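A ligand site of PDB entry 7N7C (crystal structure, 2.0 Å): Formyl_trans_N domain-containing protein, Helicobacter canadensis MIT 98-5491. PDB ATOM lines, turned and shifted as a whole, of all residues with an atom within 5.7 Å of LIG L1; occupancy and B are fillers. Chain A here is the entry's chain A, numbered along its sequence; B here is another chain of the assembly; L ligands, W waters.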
ATOM      1  N   SER A  75      28.632  19.557  25.600  1.00  0.00           N
ATOM      2  CA  SER A  75      27.394  18.963  26.169  1.00  0.00           C
ATOM      3  C   SER A  75      27.666  18.493  27.600  1.00  0.00           C
ATOM      4  O   SER A  75      28.632  17.716  27.804  1.00  0.00           O
ATOM      5  CB  SER A  75      26.864  17.861  25.287  1.00  0.00           C
ATOM      6  OG  SER A  75      25.994  17.023  26.018  1.00  0.00           O
ATOM      7  N   PHE A  78      23.228  17.247  28.159  1.00  0.00           N
ATOM      8  CA  PHE A  78      22.357  17.712  27.052  1.00  0.00           C
ATOM      9  C   PHE A  78      21.395  16.571  26.685  1.00  0.00           C
ATOM     10  O   PHE A  78      21.830  15.403  26.683  1.00  0.00           O
ATOM     11  CB  PHE A  78      23.206  18.219  25.891  1.00  0.00           C
ATOM     12  CG  PHE A  78      22.444  18.944  24.821  1.00  0.00           C
ATOM     13  CD1 PHE A  78      21.518  19.927  25.141  1.00  0.00           C
ATOM     14  CD2 PHE A  78      22.699  18.712  23.476  1.00  0.00           C
ATOM     15  CE1 PHE A  78      20.814  20.583  24.138  1.00  0.00           C
ATOM     16  CE2 PHE A  78      22.031  19.406  22.476  1.00  0.00           C
ATOM     17  CZ  PHE A  78      21.088  20.350  22.809  1.00  0.00           C
ATOM     18  N   ASP A  79      20.152  16.913  26.345  1.00  0.00           N
ATOM     19  CA  ASP A  79      19.064  15.921  26.128  1.00  0.00           C
ATOM     20  C   ASP A  79      18.972  15.510  24.642  1.00  0.00           C
ATOM     21  O   ASP A  79      18.177  14.616  24.343  1.00  0.00           O
ATOM     22  CB  ASP A  79      17.734  16.431  26.699  1.00  0.00           C
ATOM     23  CG  ASP A  79      17.267  17.797  26.228  1.00  0.00           C
ATOM     24  OD1 ASP A  79      17.983  18.449  25.429  1.00  0.00           O
ATOM     25  OD2 ASP A  79      16.167  18.211  26.662  1.00  0.00           O
ATOM     26  N   ARG A  80      19.802  16.050  23.740  1.00  0.00           N
ATOM     27  CA  ARG A  80      19.663  15.772  22.286  1.00  0.00           C
ATOM     28  C   ARG A  80      20.929  15.187  21.654  1.00  0.00           C
ATOM     29  O   ARG A  80      22.039  15.703  21.948  1.00  0.00           O
ATOM     30  CB  ARG A  80      19.300  17.056  21.563  1.00  0.00           C
ATOM     31  CG  ARG A  80      17.955  17.647  21.973  1.00  0.00           C
ATOM     32  CD  ARG A  80      17.717  18.825  21.070  1.00  0.00           C
ATOM     33  NE  ARG A  80      17.790  20.083  21.749  1.00  0.00           N
ATOM     34  CZ  ARG A  80      17.784  21.265  21.158  1.00  0.00           C
ATOM     35  NH1 ARG A  80      17.706  21.390  19.835  1.00  0.00           N
ATOM     36  NH2 ARG A  80      17.843  22.341  21.913  1.00  0.00           N
ATOM     37  N   ILE A  81      20.768  14.177  20.800  1.00  0.00           N
ATOM     38  CA  ILE A  81      21.875  13.615  19.974  1.00  0.00           C
ATOM     39  C   ILE A  81      22.118  14.581  18.812  1.00  0.00           C
ATOM     40  O   ILE A  81      21.150  14.948  18.193  1.00  0.00           O
ATOM     41  CB  ILE A  81      21.536  12.189  19.492  1.00  0.00           C
ATOM     42  CG1 ILE A  81      21.675  11.190  20.640  1.00  0.00           C
ATOM     43  CG2 ILE A  81      22.426  11.794  18.306  1.00  0.00           C
ATOM     44  CD1 ILE A  81      20.665  10.066  20.600  1.00  0.00           C
ATOM     45  N   VAL A  82      23.345  15.002  18.584  1.00  0.00           N
ATOM     46  CA  VAL A  82      23.721  15.954  17.504  1.00  0.00           C
ATOM     47  C   VAL A  82      24.280  15.144  16.316  1.00  0.00           C
ATOM     48  O   VAL A  82      24.806  14.012  16.511  1.00  0.00           O
ATOM     49  CB  VAL A  82      24.714  17.036  17.994  1.00  0.00           C
ATOM     50  CG1 VAL A  82      24.170  17.799  19.183  1.00  0.00           C
ATOM     51  CG2 VAL A  82      26.088  16.488  18.322  1.00  0.00           C
ATOM     52  N   LYS A  83      24.064  15.679  15.106  1.00  0.00           N
ATOM     53  CA  LYS A  83      24.691  15.215  13.840  1.00  0.00           C
ATOM     54  C   LYS A  83      25.944  16.070  13.587  1.00  0.00           C
ATOM     55  O   LYS A  83      25.812  17.253  13.255  1.00  0.00           O
ATOM     56  CB  LYS A  83      23.696  15.315  12.683  1.00  0.00           C
ATOM     57  CG  LYS A  83      22.616  14.241  12.660  1.00  0.00           C
ATOM     58  CD  LYS A  83      22.073  13.995  11.249  1.00  0.00           C
ATOM     59  CE  LYS A  83      20.561  14.016  11.160  1.00  0.00           C
ATOM     60  NZ  LYS A  83      19.943  12.905  11.925  1.00  0.00           N
ATOM     61  N   VAL A  84      27.106  15.477  13.771  1.00  0.00           N
ATOM     62  CA  VAL A  84      28.411  16.199  13.800  1.00  0.00           C
ATOM     63  C   VAL A  84      28.724  16.829  12.432  1.00  0.00           C
ATOM     64  O   VAL A  84      29.458  17.830  12.423  1.00  0.00           O
ATOM     65  CB  VAL A  84      29.505  15.214  14.226  1.00  0.00           C
ATOM     66  CG1 VAL A  84      30.886  15.757  13.949  1.00  0.00           C
ATOM     67  CG2 VAL A  84      29.331  14.835  15.687  1.00  0.00           C
ATOM     68  N   ASN A  94      31.711  16.175  25.114  1.00  0.00           N
ATOM     69  CA  ASN A  94      30.628  15.637  25.975  1.00  0.00           C
ATOM     70  C   ASN A  94      31.267  15.080  27.243  1.00  0.00           C
ATOM     71  O   ASN A  94      32.368  14.468  27.163  1.00  0.00           O
ATOM     72  CB  ASN A  94      29.777  14.561  25.283  1.00  0.00           C
ATOM     73  CG  ASN A  94      28.658  14.116  26.196  1.00  0.00           C
ATOM     74  OD1 ASN A  94      27.881  14.955  26.637  1.00  0.00           O
ATOM     75  ND2 ASN A  94      28.643  12.847  26.574  1.00  0.00           N
ATOM     76  N   MET A  95      30.606  15.317  28.364  1.00  0.00           N
ATOM     77  CA  MET A  95      30.877  14.627  29.633  1.00  0.00           C
ATOM     78  C   MET A  95      29.754  13.589  29.819  1.00  0.00           C
ATOM     79  O   MET A  95      28.581  13.985  29.919  1.00  0.00           O
ATOM     80  CB  MET A  95      30.872  15.631  30.795  1.00  0.00           C
ATOM     81  CG  MET A  95      31.376  15.025  32.051  1.00  0.00           C
ATOM     82  SD  MET A  95      33.144  14.713  31.982  1.00  0.00           S
ATOM     83  CE  MET A  95      33.801  16.375  32.016  1.00  0.00           C
ATOM     84  N   HIS A  96      30.130  12.319  29.801  1.00  0.00           N
ATOM     85  CA  HIS A  96      29.229  11.157  29.983  1.00  0.00           C
ATOM     86  C   HIS A  96      29.429  10.581  31.387  1.00  0.00           C
ATOM     87  O   HIS A  96      30.599  10.412  31.835  1.00  0.00           O
ATOM     88  CB  HIS A  96      29.455  10.128  28.875  1.00  0.00           C
ATOM     89  CG  HIS A  96      28.577   8.939  29.052  1.00  0.00           C
ATOM     90  ND1 HIS A  96      27.213   8.993  28.885  1.00  0.00           N
ATOM     91  CD2 HIS A  96      28.836   7.693  29.498  1.00  0.00           C
ATOM     92  CE1 HIS A  96      26.686   7.823  29.173  1.00  0.00           C
ATOM     93  NE2 HIS A  96      27.648   7.015  29.523  1.00  0.00           N
ATOM     94  N   GLY A 105      24.685   5.135  26.887  1.00  0.00           N
ATOM     95  CA  GLY A 105      23.214   5.185  26.896  1.00  0.00           C
ATOM     96  C   GLY A 105      22.734   5.970  28.092  1.00  0.00           C
ATOM     97  O   GLY A 105      23.391   6.949  28.443  1.00  0.00           O
ATOM     98  N   VAL A 106      21.637   5.544  28.723  1.00  0.00           N
ATOM     99  CA  VAL A 106      20.914   6.421  29.674  1.00  0.00           C
ATOM    100  C   VAL A 106      20.792   5.712  31.012  1.00  0.00           C
ATOM    101  O   VAL A 106      21.210   4.525  31.147  1.00  0.00           O
ATOM    102  CB  VAL A 106      19.559   6.860  29.086  1.00  0.00           C
ATOM    103  CG1 VAL A 106      19.730   7.529  27.733  1.00  0.00           C
ATOM    104  CG2 VAL A 106      18.614   5.682  28.962  1.00  0.00           C
ATOM    105  N   HIS A 125      34.828  13.034  26.454  1.00  0.00           N
ATOM    106  CA  HIS A 125      35.100  12.414  25.136  1.00  0.00           C
ATOM    107  C   HIS A 125      34.693  13.383  24.014  1.00  0.00           C
ATOM    108  O   HIS A 125      33.846  14.294  24.250  1.00  0.00           O
ATOM    109  CB  HIS A 125      34.405  11.039  25.047  1.00  0.00           C
ATOM    110  CG  HIS A 125      32.915  11.090  25.017  1.00  0.00           C
ATOM    111  ND1 HIS A 125      32.194  11.125  23.844  1.00  0.00           N
ATOM    112  CD2 HIS A 125      31.998  11.080  26.015  1.00  0.00           C
ATOM    113  CE1 HIS A 125      30.908  11.150  24.121  1.00  0.00           C
ATOM    114  NE2 HIS A 125      30.752  11.116  25.438  1.00  0.00           N
ATOM    115  N   ILE A 127      32.593  14.289  20.796  1.00  0.00           N
ATOM    116  CA  ILE A 127      31.295  13.832  20.241  1.00  0.00           C
ATOM    117  C   ILE A 127      31.571  13.271  18.843  1.00  0.00           C
ATOM    118  O   ILE A 127      32.195  13.953  18.064  1.00  0.00           O
ATOM    119  CB  ILE A 127      30.265  14.958  20.184  1.00  0.00           C
ATOM    120  CG1 ILE A 127      29.899  15.413  21.606  1.00  0.00           C
ATOM    121  CG2 ILE A 127      29.058  14.509  19.368  1.00  0.00           C
ATOM    122  CD1 ILE A 127      28.928  16.549  21.636  1.00  0.00           C
ATOM    123  N   ASP A 128      31.093  12.060  18.558  1.00  0.00           N
ATOM    124  CA  ASP A 128      30.914  11.551  17.171  1.00  0.00           C
ATOM    125  C   ASP A 128      29.427  11.252  17.037  1.00  0.00           C
ATOM    126  O   ASP A 128      28.665  11.643  17.955  1.00  0.00           O
ATOM    127  CB  ASP A 128      31.895  10.418  16.851  1.00  0.00           C
ATOM    128  CG  ASP A 128      31.664   9.103  17.598  1.00  0.00           C
ATOM    129  OD1 ASP A 128      30.565   8.848  18.065  1.00  0.00           O
ATOM    130  OD2 ASP A 128      32.598   8.337  17.655  1.00  0.00           O
ATOM    131  N   ASN A 129      29.002  10.642  15.935  1.00  0.00           N
ATOM    132  CA  ASN A 129      27.560  10.519  15.624  1.00  0.00           C
ATOM    133  C   ASN A 129      26.922   9.395  16.446  1.00  0.00           C
ATOM    134  O   ASN A 129      25.679   9.363  16.480  1.00  0.00           O
ATOM    135  CB  ASN A 129      27.311  10.281  14.136  1.00  0.00           C
ATOM    136  CG  ASN A 129      27.315  11.568  13.335  1.00  0.00           C
ATOM    137  OD1 ASN A 129      27.289  12.661  13.895  1.00  0.00           O
ATOM    138  ND2 ASN A 129      27.344  11.426  12.019  1.00  0.00           N
ATOM    139  N   GLY A 130      27.715   8.521  17.085  1.00  0.00           N
ATOM    140  CA  GLY A 130      27.129   7.462  17.925  1.00  0.00           C
ATOM    141  C   GLY A 130      26.816   7.947  19.336  1.00  0.00           C
ATOM    142  O   GLY A 130      27.280   9.041  19.724  1.00  0.00           O
ATOM    143  N   ILE A 131      26.072   7.138  20.084  1.00  0.00           N
ATOM    144  CA  ILE A 131      25.664   7.441  21.484  1.00  0.00           C
ATOM    145  C   ILE A 131      26.850   7.025  22.356  1.00  0.00           C
ATOM    146  O   ILE A 131      27.081   5.803  22.483  1.00  0.00           O
ATOM    147  CB  ILE A 131      24.356   6.740  21.836  1.00  0.00           C
ATOM    148  CG1 ILE A 131      23.215   7.155  20.897  1.00  0.00           C
ATOM    149  CG2 ILE A 131      23.967   6.999  23.281  1.00  0.00           C
ATOM    150  CD1 ILE A 131      21.957   6.340  21.076  1.00  0.00           C
ATOM    151  N   ASP A 132      27.629   8.017  22.776  1.00  0.00           N
ATOM    152  CA  ASP A 132      28.676   7.919  23.834  1.00  0.00           C
ATOM    153  C   ASP A 132      29.840   7.076  23.322  1.00  0.00           C
ATOM    154  O   ASP A 132      30.537   6.460  24.161  1.00  0.00           O
ATOM    155  CB  ASP A 132      28.099   7.376  25.144  1.00  0.00           C
ATOM    156  CG  ASP A 132      26.929   8.134  25.748  1.00  0.00           C
ATOM    157  OD1 ASP A 132      27.011   9.386  25.986  1.00  0.00           O
ATOM    158  OD2 ASP A 132      25.960   7.450  26.108  1.00  0.00           O
ATOM    159  N   THR A 133      30.103   7.141  22.007  1.00  0.00           N
ATOM    160  CA  THR A 133      31.030   6.263  21.240  1.00  0.00           C
ATOM    161  C   THR A 133      32.337   6.987  20.922  1.00  0.00           C
ATOM    162  O   THR A 133      33.332   6.277  20.625  1.00  0.00           O
ATOM    163  CB  THR A 133      30.383   5.751  19.963  1.00  0.00           C
ATOM    164  OG1 THR A 133      29.640   6.798  19.340  1.00  0.00           O
ATOM    165  CG2 THR A 133      29.481   4.579  20.272  1.00  0.00           C
ATOM    166  N   TYR A 189      25.754  -0.871  26.654  1.00  0.00           N
ATOM    167  CA  TYR A 189      24.757   0.152  26.280  1.00  0.00           C
ATOM    168  C   TYR A 189      23.414  -0.213  26.902  1.00  0.00           C
ATOM    169  O   TYR A 189      22.999  -1.378  26.869  1.00  0.00           O
ATOM    170  CB  TYR A 189      24.712   0.310  24.749  1.00  0.00           C
ATOM    171  CG  TYR A 189      23.601   1.185  24.255  1.00  0.00           C
ATOM    172  CD1 TYR A 189      23.714   2.572  24.252  1.00  0.00           C
ATOM    173  CD2 TYR A 189      22.420   0.631  23.804  1.00  0.00           C
ATOM    174  CE1 TYR A 189      22.676   3.372  23.797  1.00  0.00           C
ATOM    175  CE2 TYR A 189      21.371   1.416  23.364  1.00  0.00           C
ATOM    176  CZ  TYR A 189      21.500   2.799  23.355  1.00  0.00           C
ATOM    177  OH  TYR A 189      20.483   3.572  22.873  1.00  0.00           O
ATOM    178  N   PHE A 190      22.737   0.798  27.427  1.00  0.00           N
ATOM    179  CA  PHE A 190      21.363   0.679  27.969  1.00  0.00           C
ATOM    180  C   PHE A 190      20.530   1.859  27.467  1.00  0.00           C
ATOM    181  O   PHE A 190      20.908   3.030  27.656  1.00  0.00           O
ATOM    182  CB  PHE A 190      21.428   0.557  29.500  1.00  0.00           C
ATOM    183  CG  PHE A 190      22.121  -0.700  29.957  1.00  0.00           C
ATOM    184  CD1 PHE A 190      21.393  -1.864  30.204  1.00  0.00           C
ATOM    185  CD2 PHE A 190      23.499  -0.724  30.125  1.00  0.00           C
ATOM    186  CE1 PHE A 190      22.042  -3.040  30.592  1.00  0.00           C
ATOM    187  CE2 PHE A 190      24.135  -1.882  30.536  1.00  0.00           C
ATOM    188  CZ  PHE A 190      23.415  -3.044  30.751  1.00  0.00           C
ATOM    189  N   SER A 191      19.418   1.566  26.785  1.00  0.00           N
ATOM    190  CA  SER A 191      18.464   2.582  26.291  1.00  0.00           C
ATOM    191  C   SER A 191      17.323   2.701  27.301  1.00  0.00           C
ATOM    192  O   SER A 191      17.258   1.846  28.224  1.00  0.00           O
ATOM    193  CB  SER A 191      17.947   2.183  24.941  1.00  0.00           C
ATOM    194  OG  SER A 191      17.059   1.094  25.117  1.00  0.00           O
ATOM    195  N   ARG A 192      16.430   3.688  27.136  1.00  0.00           N
ATOM    196  CA  ARG A 192      15.303   3.916  28.079  1.00  0.00           C
ATOM    197  C   ARG A 192      14.462   2.628  28.173  1.00  0.00           C
ATOM    198  O   ARG A 192      14.020   2.309  29.286  1.00  0.00           O
ATOM    199  CB  ARG A 192      14.482   5.165  27.706  1.00  0.00           C
ATOM    200  CG  ARG A 192      15.318   6.453  27.666  1.00  0.00           C
ATOM    201  CD  ARG A 192      14.768   7.697  28.367  1.00  0.00           C
ATOM    202  NE  ARG A 192      15.708   8.396  29.277  1.00  0.00           N
ATOM    203  CZ  ARG A 192      16.496   9.423  28.970  1.00  0.00           C
ATOM    204  NH1 ARG A 192      16.512   9.908  27.737  1.00  0.00           N
ATOM    205  NH2 ARG A 192      17.271   9.967  29.918  1.00  0.00           N
ATOM    206  N   GLN A 193      14.312   1.869  27.092  1.00  0.00           N
ATOM    207  CA  GLN A 193      13.448   0.660  27.057  1.00  0.00           C
ATOM    208  C   GLN A 193      14.085  -0.480  27.863  1.00  0.00           C
ATOM    209  O   GLN A 193      13.369  -1.418  28.194  1.00  0.00           O
ATOM    210  CB  GLN A 193      13.192   0.185  25.626  1.00  0.00           C
ATOM    211  CG  GLN A 193      14.267  -0.756  25.101  1.00  0.00           C
ATOM    212  CD  GLN A 193      14.267  -0.926  23.600  1.00  0.00           C
ATOM    213  OE1 GLN A 193      13.234  -0.750  22.936  1.00  0.00           O
ATOM    214  NE2 GLN A 193      15.428  -1.264  23.047  1.00  0.00           N
ATOM    215  N   LYS B 204      19.849  -3.562  19.729  1.00  0.00           N
ATOM    216  CA  LYS B 204      20.035  -2.161  20.218  1.00  0.00           C
ATOM    217  C   LYS B 204      21.021  -2.233  21.384  1.00  0.00           C
ATOM    218  O   LYS B 204      20.716  -1.759  22.511  1.00  0.00           O
ATOM    219  CB  LYS B 204      18.719  -1.477  20.561  1.00  0.00           C
ATOM    220  CG  LYS B 204      17.916  -1.015  19.350  1.00  0.00           C
ATOM    221  CD  LYS B 204      16.437  -0.881  19.633  1.00  0.00           C
ATOM    222  CE  LYS B 204      15.575  -0.883  18.385  1.00  0.00           C
ATOM    223  NZ  LYS B 204      15.479   0.477  17.818  1.00  0.00           N
HETATM  224  N1  LIG L   1      25.383  13.565  20.419  1.00  0.00           N
HETATM  225  C1  LIG L   1      26.042  12.532  19.820  1.00  0.00           C
HETATM  226  N2  LIG L   1      26.065  12.483  18.485  1.00  0.00           N
HETATM  227  N3  LIG L   1      26.710  11.627  20.532  1.00  0.00           N
HETATM  228  C2  LIG L   1      26.696  11.689  21.919  1.00  0.00           C
HETATM  229  O1  LIG L   1      27.318  10.817  22.516  1.00  0.00           O
HETATM  230  C3  LIG L   1      26.018  12.757  22.598  1.00  0.00           C
HETATM  231  N4  LIG L   1      25.854  12.841  24.030  1.00  0.00           N
HETATM  232  C4  LIG L   1      24.764  13.775  24.498  1.00  0.00           C
HETATM  233  C5  LIG L   1      24.850  15.080  23.720  1.00  0.00           C
HETATM  234  N5  LIG L   1      24.706  14.785  22.316  1.00  0.00           N
HETATM  235  C6  LIG L   1      25.359  13.709  21.780  1.00  0.00           C
HETATM  236  C7  LIG L   1      23.340  13.202  24.308  1.00  0.00           C
HETATM  237  N6  LIG L   1      23.022  11.937  24.956  1.00  0.00           N
HETATM  238  C8  LIG L   1      19.538   9.804  24.044  1.00  0.00           C
HETATM  239  C9  LIG L   1      19.633  11.179  23.841  1.00  0.00           C
HETATM  240  C10 LIG L   1      20.775  11.874  24.166  1.00  0.00           C
HETATM  241  C11 LIG L   1      21.886  11.211  24.669  1.00  0.00           C
HETATM  242  C12 LIG L   1      21.807   9.833  24.866  1.00  0.00           C
HETATM  243  C13 LIG L   1      20.663   9.141  24.550  1.00  0.00           C
HETATM  244  C14 LIG L   1      18.246   9.156  23.640  1.00  0.00           C
HETATM  245  O2  LIG L   1      17.321   9.836  23.209  1.00  0.00           O
HETATM  246  N7  LIG L   1      18.173   7.816  23.744  1.00  0.00           N
HETATM  247  C15 LIG L   1      17.031   7.021  23.272  1.00  0.00           C
HETATM  248  C16 LIG L   1      17.375   6.199  22.015  1.00  0.00           C
HETATM  249  C17 LIG L   1      17.263   6.962  20.708  1.00  0.00           C
HETATM  250  C18 LIG L   1      17.942   6.235  19.558  1.00  0.00           C
HETATM  251  O3  LIG L   1      17.943   4.981  19.587  1.00  0.00           O
HETATM  252  O4  LIG L   1      18.537   6.905  18.688  1.00  0.00           O
HETATM  253  C19 LIG L   1      16.616   6.027  24.371  1.00  0.00           C
HETATM  254  O5  LIG L   1      17.490   5.674  25.173  1.00  0.00           O
HETATM  255  O6  LIG L   1      15.472   5.555  24.307  1.00  0.00           O
HETATM  256  C20 LIG L   1      26.396  12.081  25.049  1.00  0.00           C
HETATM  257  O7  LIG L   1      25.798  11.826  26.141  1.00  0.00           O
HETATM  258  O1  LG2 L   2      12.536   8.365  35.561  1.00  0.00           O
HETATM  259  C1  LG2 L   2      13.649   8.543  36.002  1.00  0.00           C
HETATM  260  N1  LG2 L   2      14.057   7.896  37.085  1.00  0.00           N
HETATM  261  C2  LG2 L   2      15.273   8.075  37.584  1.00  0.00           C
HETATM  262  O2  LG2 L   2      15.576   7.450  38.554  1.00  0.00           O
HETATM  263  C3  LG2 L   2      14.520   9.420  35.422  1.00  0.00           C
HETATM  264  C4  LG2 L   2      14.109  10.170  34.216  1.00  0.00           C
HETATM  265  C5  LG2 L   2      15.782   9.581  35.941  1.00  0.00           C
HETATM  266  N2  LG2 L   2      16.175   8.945  36.993  1.00  0.00           N
HETATM  267  C6  LG2 L   2      17.488   9.115  37.542  1.00  0.00           C
HETATM  268  O3  LG2 L   2      18.089  10.339  37.271  1.00  0.00           O
HETATM  269  C7  LG2 L   2      18.412   8.062  36.962  1.00  0.00           C
HETATM  270  C8  LG2 L   2      19.221   8.801  35.947  1.00  0.00           C
HETATM  271  O4  LG2 L   2      20.492   8.218  35.728  1.00  0.00           O
HETATM  272  C9  LG2 L   2      19.279  10.169  36.553  1.00  0.00           C
HETATM  273  C10 LG2 L   2      19.431  11.238  35.513  1.00  0.00           C
HETATM  274  O5  LG2 L   2      18.354  11.252  34.652  1.00  0.00           O
HETATM  275  P1  LG2 L   2      18.464  11.896  33.284  1.00  0.00           P
HETATM  276  O6  LG2 L   2      18.679  13.245  33.467  1.00  0.00           O
HETATM  277  O7  LG2 L   2      17.328  11.614  32.514  1.00  0.00           O
HETATM  278  O8  LG2 L   2      19.794  11.380  32.682  1.00  0.00           O
HETATM  279  P2  LG2 L   2      20.224   9.938  32.261  1.00  0.00           P
HETATM  280  O9  LG2 L   2      19.118   9.189  31.756  1.00  0.00           O
HETATM  281  O10 LG2 L   2      20.984   9.345  33.295  1.00  0.00           O
HETATM  282  O11 LG2 L   2      21.303  10.243  31.131  1.00  0.00           O
HETATM  283  O12 LG2 L   2      22.327  14.243  28.803  1.00  0.00           O
HETATM  284  C11 LG2 L   2      21.812  12.950  28.778  1.00  0.00           C
HETATM  285  C12 LG2 L   2      20.747  12.799  29.833  1.00  0.00           C
HETATM  286  O13 LG2 L   2      20.138  11.534  29.617  1.00  0.00           O
HETATM  287  C13 LG2 L   2      19.757  13.943  29.789  1.00  0.00           C
HETATM  288  C14 LG2 L   2      22.913  12.009  29.164  1.00  0.00           C
HETATM  289  N3  LG2 L   2      24.139  12.241  28.403  1.00  0.00           N
HETATM  290  C15 LG2 L   2      22.348  10.622  28.956  1.00  0.00           C
HETATM  291  O14 LG2 L   2      23.288   9.690  29.410  1.00  0.00           O
HETATM  292  C16 LG2 L   2      21.028  10.468  29.738  1.00  0.00           C
HETATM  293  O   HOH W   1      14.616   2.963  24.381  1.00  0.00           O
HETATM  294  O   HOH W   2      18.774   2.615  21.428  1.00  0.00           O
HETATM  295  O   HOH W   3      15.566   4.331  17.802  1.00  0.00           O
HETATM  296  O   HOH W   4      29.853  10.215  20.717  1.00  0.00           O
HETATM  297  O   HOH W   5      20.055   5.673  24.517  1.00  0.00           O
HETATM  298  O   HOH W   6      24.274   9.364  26.632  1.00  0.00           O
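The backbone carbonyl oxygen (O) of Gly 105 sits at hydrogen-bond distance from an oxygen (O14) of LG2 L2, 2.9 Å away.
An oxygen (O7) of LIG L1 lies close to the side-chain carboxylate of Asp 132 (2.7 Å).
The guanidinium group of Arg 192 lies within salt-bridge range of an oxygen (O9) of LG2 L2 (2.7 Å).
The backbone carbonyl oxygen of Arg 80 lies within hydrogen-bond range of a nitrogen (N5) of LIG L1, at 2.8 Å.
The backbone NH (N) of Arg 192 lies within hydrogen-bond range of an oxygen (O5) of LIG L1.
The backbone NH (N) of Asp 132 sits at hydrogen-bond distance from an oxygen (O1) of LIG L1 (2.8 Å).
The backbone carbonyl oxygen of Gly 130 lies close to a nitrogen (N3) of LIG L1, at 2.8 Å.
The backbone carbonyl oxygen (O) of Val 82 sits at hydrogen-bond distance from a nitrogen (N2) of LIG L1 (2.8 Å).
The backbone carbonyl oxygen of Phe 78 is in hydrogen-bond range of an oxygen (O12) of LG2 L2, at 2.5 Å.
The backbone carbonyl oxygen (O) of Asp 128 is in hydrogen-bond range of a nitrogen (N2) of LIG L1 (2.8 Å).
The backbone NH (N) of Val 82 is in hydrogen-bond range of a nitrogen (N1) of LIG L1.
The side-chain amide nitrogen (ND2) of Asn 94 sits close to an oxygen (O7) of LIG L1.
O12 of LG2 L2 lies within hydrogen-bond range of N of Phe 78, 3.2 Å away.
A nitrogen (N3) of LG2 L2 sits at hydrogen-bond distance from an oxygen (O7) of LIG L1.
The backbone carbonyl oxygen (O) of Phe 190 lies within hydrogen-bond range of the backbone NH (N) of Val 106 (2.8 Å).
The side-chain carboxylate (OD1) of Asp 128 lies within hydrogen-bond range of the side-chain hydroxyl (OG1) of Thr 133.
The side-chain carboxylate (OD1) of Asp 132 sits at hydrogen-bond distance from a ring nitrogen (ND1) of His 96 (2.9 Å).
The backbone NH (N) of His 125 lies within hydrogen-bond range of the backbone carbonyl oxygen (O) of Asn 94, 2.9 Å away.
N of Gln 193 sits close to OG of Ser 191, at 3.5 Å.
O of Gly 130 sits close to OG1 of Thr 133 (3.3 Å).
The side-chain carboxylate (OD2) of Asp 132 is in hydrogen-bond range of the backbone NH (N) of Gly 105, 2.8 Å away.
The side-chain hydroxyl of Ser 75 is in hydrogen-bond range of the side-chain amide oxygen of Asn 94, 2.9 Å away.
OG of Ser 75 touches C5 of LIG L1, 3.2 Å away.
O of Phe 78 touches C7 of LIG L1, at 3.6 Å.
O of Asp 79 touches C9 of LIG L1, 3.8 Å away.
Ile 81 touches LIG L1 (CA to N1, 3.5 Å).
CG1 of Val 106 touches C13 of LIG L1, at 3.7 Å.
His 125 touches LIG L1 (CE1 to O1, 3.9 Å).
Ile 127 touches LIG L1 (CG2 to C1, 3.6 Å).
Asn 129 touches LIG L1.
C of Ile 131 touches O1 of LIG L1, at 3.8 Å.
Ser 191 touches LIG L1.
Within 4 Å of LIG L1: Ser 75, Phe 78, Asp 79, Arg 80, Ile 81, Val 82, Asn 94, Val 106, His 125, Ile 127, Asp 128, Asn 129, Gly 130, Ile 131, Asp 132, Ser 191 and Arg 192.
The nearest printed residue that does not touch LIG L1 is Tyr 189 (4.2 Å).
Water W5 bridges O5 of LIG L1 (2.6 Å) and OH of Tyr 189 (2.7 Å).
Water W1 lies within hydrogen-bond range of an oxygen (O6) of LIG L1 (2.7 Å), the backbone NH (N) of Gln 193 (2.9 Å), the side-chain hydroxyl (OG) of Ser 191 (3.2 Å) and the backbone NH (N) of Arg 192 (3.4 Å).
Water W2 bridges OH of Tyr 189 (2.4 Å) and O3 of LIG L1 (3.1 Å).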
